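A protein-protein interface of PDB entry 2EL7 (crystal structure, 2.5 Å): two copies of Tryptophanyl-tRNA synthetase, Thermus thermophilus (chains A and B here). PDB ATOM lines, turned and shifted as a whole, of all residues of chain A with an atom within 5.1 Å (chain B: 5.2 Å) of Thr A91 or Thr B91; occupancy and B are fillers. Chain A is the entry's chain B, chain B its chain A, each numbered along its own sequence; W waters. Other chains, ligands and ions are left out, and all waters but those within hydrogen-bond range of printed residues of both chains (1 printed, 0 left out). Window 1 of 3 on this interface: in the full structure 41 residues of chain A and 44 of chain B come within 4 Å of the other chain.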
ATOM      1  N   TYR A  44      -9.108 -17.243  -3.829  1.00  0.00           N
ATOM      2  CA  TYR A  44      -9.028 -16.066  -4.706  1.00  0.00           C
ATOM      3  C   TYR A  44      -7.664 -15.932  -5.388  1.00  0.00           C
ATOM      4  O   TYR A  44      -7.511 -15.179  -6.354  1.00  0.00           O
ATOM      5  CB  TYR A  44      -9.410 -14.772  -3.945  1.00  0.00           C
ATOM      6  CG  TYR A  44     -10.852 -14.334  -4.192  1.00  0.00           C
ATOM      7  CD1 TYR A  44     -11.607 -13.674  -3.201  1.00  0.00           C
ATOM      8  CD2 TYR A  44     -11.474 -14.604  -5.408  1.00  0.00           C
ATOM      9  CE1 TYR A  44     -12.966 -13.306  -3.426  1.00  0.00           C
ATOM     10  CE2 TYR A  44     -12.820 -14.244  -5.647  1.00  0.00           C
ATOM     11  CZ  TYR A  44     -13.561 -13.605  -4.663  1.00  0.00           C
ATOM     12  OH  TYR A  44     -14.893 -13.309  -4.942  1.00  0.00           O
ATOM     13  N   PRO A  88     -15.864 -11.955   2.633  1.00  0.00           N
ATOM     14  CA  PRO A  88     -15.671 -10.847   1.690  1.00  0.00           C
ATOM     15  C   PRO A  88     -15.075  -9.550   2.239  1.00  0.00           C
ATOM     16  O   PRO A  88     -14.487  -8.754   1.492  1.00  0.00           O
ATOM     17  CB  PRO A  88     -17.078 -10.636   1.145  1.00  0.00           C
ATOM     18  CG  PRO A  88     -17.920 -10.857   2.381  1.00  0.00           C
ATOM     19  CD  PRO A  88     -17.306 -12.163   2.888  1.00  0.00           C
ATOM     20  N   GLU A  89     -15.250  -9.312   3.528  1.00  0.00           N
ATOM     21  CA  GLU A  89     -14.717  -8.098   4.114  1.00  0.00           C
ATOM     22  C   GLU A  89     -13.263  -7.834   3.732  1.00  0.00           C
ATOM     23  O   GLU A  89     -12.853  -6.686   3.560  1.00  0.00           O
ATOM     24  CB  GLU A  89     -14.795  -8.148   5.645  1.00  0.00           C
ATOM     25  CG  GLU A  89     -16.138  -7.837   6.259  1.00  0.00           C
ATOM     26  CD  GLU A  89     -17.165  -8.883   5.969  1.00  0.00           C
ATOM     27  OE1 GLU A  89     -16.801 -10.069   5.845  1.00  0.00           O
ATOM     28  OE2 GLU A  89     -18.350  -8.519   5.883  1.00  0.00           O
ATOM     29  N   HIS A  90     -12.458  -8.867   3.569  1.00  0.00           N
ATOM     30  CA  HIS A  90     -11.084  -8.524   3.295  1.00  0.00           C
ATOM     31  C   HIS A  90     -10.776  -7.949   1.938  1.00  0.00           C
ATOM     32  O   HIS A  90      -9.714  -7.376   1.777  1.00  0.00           O
ATOM     33  CB  HIS A  90     -10.129  -9.678   3.629  1.00  0.00           C
ATOM     34  CG  HIS A  90      -9.845 -10.585   2.484  1.00  0.00           C
ATOM     35  ND1 HIS A  90     -10.664 -11.638   2.154  1.00  0.00           N
ATOM     36  CD2 HIS A  90      -8.846 -10.573   1.570  1.00  0.00           C
ATOM     37  CE1 HIS A  90     -10.180 -12.237   1.079  1.00  0.00           C
ATOM     38  NE2 HIS A  90      -9.077 -11.609   0.706  1.00  0.00           N
ATOM     39  N   THR A  91     -11.668  -8.073   0.959  1.00  0.00           N
ATOM     40  CA  THR A  91     -11.366  -7.457  -0.330  1.00  0.00           C
ATOM     41  C   THR A  91     -11.623  -5.963  -0.195  1.00  0.00           C
ATOM     42  O   THR A  91     -11.060  -5.151  -0.937  1.00  0.00           O
ATOM     43  CB  THR A  91     -12.237  -7.985  -1.486  1.00  0.00           C
ATOM     44  OG1 THR A  91     -13.618  -7.706  -1.219  1.00  0.00           O
ATOM     45  CG2 THR A  91     -11.999  -9.462  -1.690  1.00  0.00           C
ATOM     46  N   GLU A  92     -12.496  -5.607   0.745  1.00  0.00           N
ATOM     47  CA  GLU A  92     -12.794  -4.211   0.987  1.00  0.00           C
ATOM     48  C   GLU A  92     -11.576  -3.604   1.656  1.00  0.00           C
ATOM     49  O   GLU A  92     -11.170  -2.498   1.328  1.00  0.00           O
ATOM     50  CB  GLU A  92     -14.016  -4.043   1.892  1.00  0.00           C
ATOM     51  CG  GLU A  92     -14.291  -2.578   2.217  1.00  0.00           C
ATOM     52  CD  GLU A  92     -15.416  -2.383   3.213  1.00  0.00           C
ATOM     53  OE1 GLU A  92     -15.628  -1.222   3.645  1.00  0.00           O
ATOM     54  OE2 GLU A  92     -16.090  -3.381   3.558  1.00  0.00           O
ATOM     55  N   LEU A  93     -10.992  -4.324   2.605  1.00  0.00           N
ATOM     56  CA  LEU A  93      -9.806  -3.832   3.305  1.00  0.00           C
ATOM     57  C   LEU A  93      -8.668  -3.763   2.292  1.00  0.00           C
ATOM     58  O   LEU A  93      -7.773  -2.905   2.378  1.00  0.00           O
ATOM     59  CB  LEU A  93      -9.434  -4.771   4.462  1.00  0.00           C
ATOM     60  CG  LEU A  93      -8.177  -4.414   5.263  1.00  0.00           C
ATOM     61  CD1 LEU A  93      -8.294  -2.990   5.881  1.00  0.00           C
ATOM     62  CD2 LEU A  93      -7.998  -5.460   6.341  1.00  0.00           C
ATOM     63  N   SER A  94      -8.736  -4.655   1.309  1.00  0.00           N
ATOM     64  CA  SER A  94      -7.730  -4.713   0.259  1.00  0.00           C
ATOM     65  C   SER A  94      -7.677  -3.406  -0.555  1.00  0.00           C
ATOM     66  O   SER A  94      -6.592  -2.935  -0.950  1.00  0.00           O
ATOM     67  CB  SER A  94      -8.028  -5.907  -0.647  1.00  0.00           C
ATOM     68  OG  SER A  94      -6.973  -6.132  -1.553  1.00  0.00           O
ATOM     69  N   TRP A  95      -8.842  -2.815  -0.819  1.00  0.00           N
ATOM     70  CA  TRP A  95      -8.861  -1.558  -1.567  1.00  0.00           C
ATOM     71  C   TRP A  95      -8.193  -0.503  -0.730  1.00  0.00           C
ATOM     72  O   TRP A  95      -7.420   0.285  -1.243  1.00  0.00           O
ATOM     73  CB  TRP A  95     -10.285  -1.082  -1.894  1.00  0.00           C
ATOM     74  CG  TRP A  95     -10.319   0.394  -2.263  1.00  0.00           C
ATOM     75  CD1 TRP A  95     -10.905   1.403  -1.548  1.00  0.00           C
ATOM     76  CD2 TRP A  95      -9.659   1.026  -3.378  1.00  0.00           C
ATOM     77  NE1 TRP A  95     -10.651   2.626  -2.146  1.00  0.00           N
ATOM     78  CE2 TRP A  95      -9.888   2.422  -3.267  1.00  0.00           C
ATOM     79  CE3 TRP A  95      -8.897   0.548  -4.453  1.00  0.00           C
ATOM     80  CZ2 TRP A  95      -9.381   3.346  -4.189  1.00  0.00           C
ATOM     81  CZ3 TRP A  95      -8.387   1.465  -5.378  1.00  0.00           C
ATOM     82  CH2 TRP A  95      -8.633   2.856  -5.235  1.00  0.00           C
ATOM     83  N   LEU A 132      -3.564  -8.121  -1.498  1.00  0.00           N
ATOM     84  CA  LEU A 132      -4.711  -8.922  -1.046  1.00  0.00           C
ATOM     85  C   LEU A 132      -4.281  -9.808   0.126  1.00  0.00           C
ATOM     86  O   LEU A 132      -5.057 -10.052   1.055  1.00  0.00           O
ATOM     87  CB  LEU A 132      -5.256  -9.802  -2.186  1.00  0.00           C
ATOM     88  CG  LEU A 132      -6.460 -10.685  -1.821  1.00  0.00           C
ATOM     89  CD1 LEU A 132      -7.627  -9.775  -1.428  1.00  0.00           C
ATOM     90  CD2 LEU A 132      -6.858 -11.588  -3.017  1.00  0.00           C
ATOM     91  N   TYR B  44     -14.785   6.590  -1.637  1.00  0.00           N
ATOM     92  CA  TYR B  44     -13.548   5.823  -1.773  1.00  0.00           C
ATOM     93  C   TYR B  44     -12.521   6.504  -2.676  1.00  0.00           C
ATOM     94  O   TYR B  44     -11.340   6.191  -2.599  1.00  0.00           O
ATOM     95  CB  TYR B  44     -13.832   4.413  -2.306  1.00  0.00           C
ATOM     96  CG  TYR B  44     -14.132   3.412  -1.204  1.00  0.00           C
ATOM     97  CD1 TYR B  44     -14.938   2.294  -1.442  1.00  0.00           C
ATOM     98  CD2 TYR B  44     -13.624   3.594   0.079  1.00  0.00           C
ATOM     99  CE1 TYR B  44     -15.238   1.389  -0.422  1.00  0.00           C
ATOM    100  CE2 TYR B  44     -13.912   2.693   1.109  1.00  0.00           C
ATOM    101  CZ  TYR B  44     -14.718   1.596   0.853  1.00  0.00           C
ATOM    102  OH  TYR B  44     -15.010   0.717   1.879  1.00  0.00           O
ATOM    103  N   PRO B  88     -20.319  -2.360  -0.074  1.00  0.00           N
ATOM    104  CA  PRO B  88     -18.976  -2.931  -0.179  1.00  0.00           C
ATOM    105  C   PRO B  88     -18.735  -4.046  -1.194  1.00  0.00           C
ATOM    106  O   PRO B  88     -17.580  -4.308  -1.538  1.00  0.00           O
ATOM    107  CB  PRO B  88     -18.710  -3.385   1.252  1.00  0.00           C
ATOM    108  CG  PRO B  88     -20.073  -3.939   1.634  1.00  0.00           C
ATOM    109  CD  PRO B  88     -20.972  -2.799   1.177  1.00  0.00           C
ATOM    110  N   GLU B  89     -19.806  -4.707  -1.647  1.00  0.00           N
ATOM    111  CA  GLU B  89     -19.709  -5.787  -2.620  1.00  0.00           C
ATOM    112  C   GLU B  89     -18.849  -5.403  -3.828  1.00  0.00           C
ATOM    113  O   GLU B  89     -18.119  -6.233  -4.361  1.00  0.00           O
ATOM    114  CB  GLU B  89     -21.100  -6.189  -3.165  1.00  0.00           C
ATOM    115  CG  GLU B  89     -21.997  -7.084  -2.316  1.00  0.00           C
ATOM    116  CD  GLU B  89     -22.556  -6.398  -1.094  1.00  0.00           C
ATOM    117  OE1 GLU B  89     -22.673  -5.157  -1.086  1.00  0.00           O
ATOM    118  OE2 GLU B  89     -22.901  -7.107  -0.132  1.00  0.00           O
ATOM    119  N   HIS B  90     -18.929  -4.158  -4.289  1.00  0.00           N
ATOM    120  CA  HIS B  90     -18.142  -3.840  -5.458  1.00  0.00           C
ATOM    121  C   HIS B  90     -16.646  -3.977  -5.268  1.00  0.00           C
ATOM    122  O   HIS B  90     -15.941  -4.203  -6.254  1.00  0.00           O
ATOM    123  CB  HIS B  90     -18.525  -2.458  -6.061  1.00  0.00           C
ATOM    124  CG  HIS B  90     -17.876  -1.280  -5.404  1.00  0.00           C
ATOM    125  ND1 HIS B  90     -18.349  -0.726  -4.235  1.00  0.00           N
ATOM    126  CD2 HIS B  90     -16.784  -0.563  -5.749  1.00  0.00           C
ATOM    127  CE1 HIS B  90     -17.570   0.282  -3.885  1.00  0.00           C
ATOM    128  NE2 HIS B  90     -16.613   0.401  -4.789  1.00  0.00           N
ATOM    129  N   THR B  91     -16.143  -3.872  -4.034  1.00  0.00           N
ATOM    130  CA  THR B  91     -14.698  -4.040  -3.839  1.00  0.00           C
ATOM    131  C   THR B  91     -14.326  -5.478  -4.040  1.00  0.00           C
ATOM    132  O   THR B  91     -13.163  -5.794  -4.224  1.00  0.00           O
ATOM    133  CB  THR B  91     -14.137  -3.626  -2.400  1.00  0.00           C
ATOM    134  OG1 THR B  91     -14.695  -4.455  -1.371  1.00  0.00           O
ATOM    135  CG2 THR B  91     -14.388  -2.166  -2.123  1.00  0.00           C
ATOM    136  N   GLU B  92     -15.306  -6.362  -3.958  1.00  0.00           N
ATOM    137  CA  GLU B  92     -15.043  -7.781  -4.151  1.00  0.00           C
ATOM    138  C   GLU B  92     -15.014  -8.075  -5.658  1.00  0.00           C
ATOM    139  O   GLU B  92     -14.136  -8.797  -6.161  1.00  0.00           O
ATOM    140  CB  GLU B  92     -16.113  -8.610  -3.479  1.00  0.00           C
ATOM    141  CG  GLU B  92     -15.867 -10.085  -3.608  1.00  0.00           C
ATOM    142  CD  GLU B  92     -17.010 -10.903  -3.077  1.00  0.00           C
ATOM    143  OE1 GLU B  92     -17.844 -10.322  -2.360  1.00  0.00           O
ATOM    144  OE2 GLU B  92     -17.071 -12.125  -3.370  1.00  0.00           O
ATOM    145  N   LEU B  93     -15.982  -7.501  -6.370  1.00  0.00           N
ATOM    146  CA  LEU B  93     -16.063  -7.644  -7.811  1.00  0.00           C
ATOM    147  C   LEU B  93     -14.773  -7.012  -8.329  1.00  0.00           C
ATOM    148  O   LEU B  93     -14.216  -7.408  -9.364  1.00  0.00           O
ATOM    149  CB  LEU B  93     -17.271  -6.866  -8.344  1.00  0.00           C
ATOM    150  CG  LEU B  93     -17.416  -6.900  -9.857  1.00  0.00           C
ATOM    151  CD1 LEU B  93     -17.352  -8.358 -10.324  1.00  0.00           C
ATOM    152  CD2 LEU B  93     -18.756  -6.269 -10.248  1.00  0.00           C
ATOM    153  N   SER B  94     -14.298  -6.028  -7.570  1.00  0.00           N
ATOM    154  CA  SER B  94     -13.081  -5.301  -7.926  1.00  0.00           C
ATOM    155  C   SER B  94     -11.849  -6.212  -8.012  1.00  0.00           C
ATOM    156  O   SER B  94     -10.979  -6.038  -8.882  1.00  0.00           O
ATOM    157  CB  SER B  94     -12.834  -4.194  -6.908  1.00  0.00           C
ATOM    158  OG  SER B  94     -11.946  -3.257  -7.444  1.00  0.00           O
ATOM    159  N   TRP B  95     -11.767  -7.176  -7.104  1.00  0.00           N
ATOM    160  CA  TRP B  95     -10.639  -8.092  -7.128  1.00  0.00           C
ATOM    161  C   TRP B  95     -10.734  -8.935  -8.384  1.00  0.00           C
ATOM    162  O   TRP B  95      -9.735  -9.107  -9.091  1.00  0.00           O
ATOM    163  CB  TRP B  95     -10.613  -8.998  -5.886  1.00  0.00           C
ATOM    164  CG  TRP B  95      -9.674 -10.158  -6.065  1.00  0.00           C
ATOM    165  CD1 TRP B  95     -10.000 -11.483  -6.076  1.00  0.00           C
ATOM    166  CD2 TRP B  95      -8.265 -10.095  -6.325  1.00  0.00           C
ATOM    167  NE1 TRP B  95      -8.882 -12.251  -6.330  1.00  0.00           N
ATOM    168  CE2 TRP B  95      -7.805 -11.423  -6.483  1.00  0.00           C
ATOM    169  CE3 TRP B  95      -7.344  -9.048  -6.439  1.00  0.00           C
ATOM    170  CZ2 TRP B  95      -6.473 -11.728  -6.744  1.00  0.00           C
ATOM    171  CZ3 TRP B  95      -6.008  -9.357  -6.700  1.00  0.00           C
ATOM    172  CH2 TRP B  95      -5.591 -10.683  -6.849  1.00  0.00           C
ATOM    173  N   LEU B 132     -11.666  -0.084  -9.896  1.00  0.00           N
ATOM    174  CA  LEU B 132     -12.679   0.142  -8.867  1.00  0.00           C
ATOM    175  C   LEU B 132     -13.919   0.762  -9.519  1.00  0.00           C
ATOM    176  O   LEU B 132     -15.038   0.317  -9.266  1.00  0.00           O
ATOM    177  CB  LEU B 132     -12.154   1.083  -7.783  1.00  0.00           C
ATOM    178  CG  LEU B 132     -13.035   1.295  -6.542  1.00  0.00           C
ATOM    179  CD1 LEU B 132     -13.175   0.001  -5.827  1.00  0.00           C
ATOM    180  CD2 LEU B 132     -12.414   2.326  -5.594  1.00  0.00           C
HETATM  181  O   HOH W   1     -16.216  -6.423  -0.122  1.00  0.00           O
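The side-chain carboxylate of Glu A92 lies within hydrogen-bond range of the side-chain hydroxyl of Tyr B44 (2.7 Å). The side-chain hydroxyl of Thr A91 lies within hydrogen-bond range of the side-chain hydroxyl of Thr B91 (3.4 Å). OG1 of Thr B91 sits close to N of Glu A92 (3.3 Å). OE2 of Glu B92 lies within hydrogen-bond range of OH of Tyr A44 (2.9 Å). The side-chain hydroxyl of Thr A91 lies close to the backbone NH of Glu B92. The indole nitrogen of Trp B95 sits at hydrogen-bond distance from the backbone carbonyl oxygen of Tyr A44 (3.2 Å).
The side-chain hydroxyl of Thr B91 sits at hydrogen-bond distance from the backbone carbonyl oxygen of Pro B88 (2.9 Å). OG1 of Thr A91 is in hydrogen-bond range of O of Pro A88 (3.0 Å).
Among the printed residues, merely in contact across the chains: Pro A88 with Glu B92 (3.6 Å), Glu A92 with Pro B88 (3.5 Å), Trp A95 with Tyr B44 (3.7 Å), Trp A95 with Leu B132 (3.4 Å) and Leu A132 with Trp B95 (3.6 Å).
Printed residues of chain B within 4 Å of Thr A91: Thr B91 (3.4 Å) and Glu B92 (3.3 Å). Of chain A, only Thr A91 and Glu A92 come within 4 Å of Thr B91. Printed residues of chain B within 4 Å of Glu A92: Tyr B44 (2.7 Å), Pro B88 (3.5 Å) and Thr B91 (3.0 Å). Printed residues of chain B within 4 Å of Pro A88: Glu B92. Printed residues of chain B within 4 Å of Leu A132: Trp B95. Printed residues of chain B within 4 Å of Tyr A44: Glu B92 (2.9 Å) and Trp B95 (3.2 Å). Glu A89 touches none of the printed residues of chain B. The nearest residue of chain B that does not touch Thr A91 is Trp B95 (4.4 Å).
Printed residues of chain B that touch a printed residue of chain A: Tyr B44, Pro B88, Thr B91, Glu B92, Trp B95 and Leu B132. Hydrophobic or aromatic side chains of chain B within 4 Å of the printed part of chain A: Tyr B44, Pro B88, Trp B95 and Leu B132. Among the printed residues, no Asp or Glu carboxylate lies within 4 Å of a Lys or Arg side-chain nitrogen of the other chain.
Tyr A44 touches Glu B92, and with the chains exchanged Glu A92 touches Tyr B44. Tyr A44 touches Trp B95, and with the chains exchanged Trp A95 touches Tyr B44. Pro A88 touches Glu B92, and with the chains exchanged Glu A92 touches Pro B88. Thr A91 touches Glu B92, and with the chains exchanged Glu A92 touches Thr B91. Of the 11 pairs that touch across the chains among the printed residues, 11 have their exchanged pair printed and touching as well.
Water W1 lies within hydrogen-bond range of OG1 of Thr B91 (2.8 Å), O of Pro B88 (2.9 Å), OG1 of Thr A91 (3.1 Å) and O of Pro A88 (3.3 Å).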
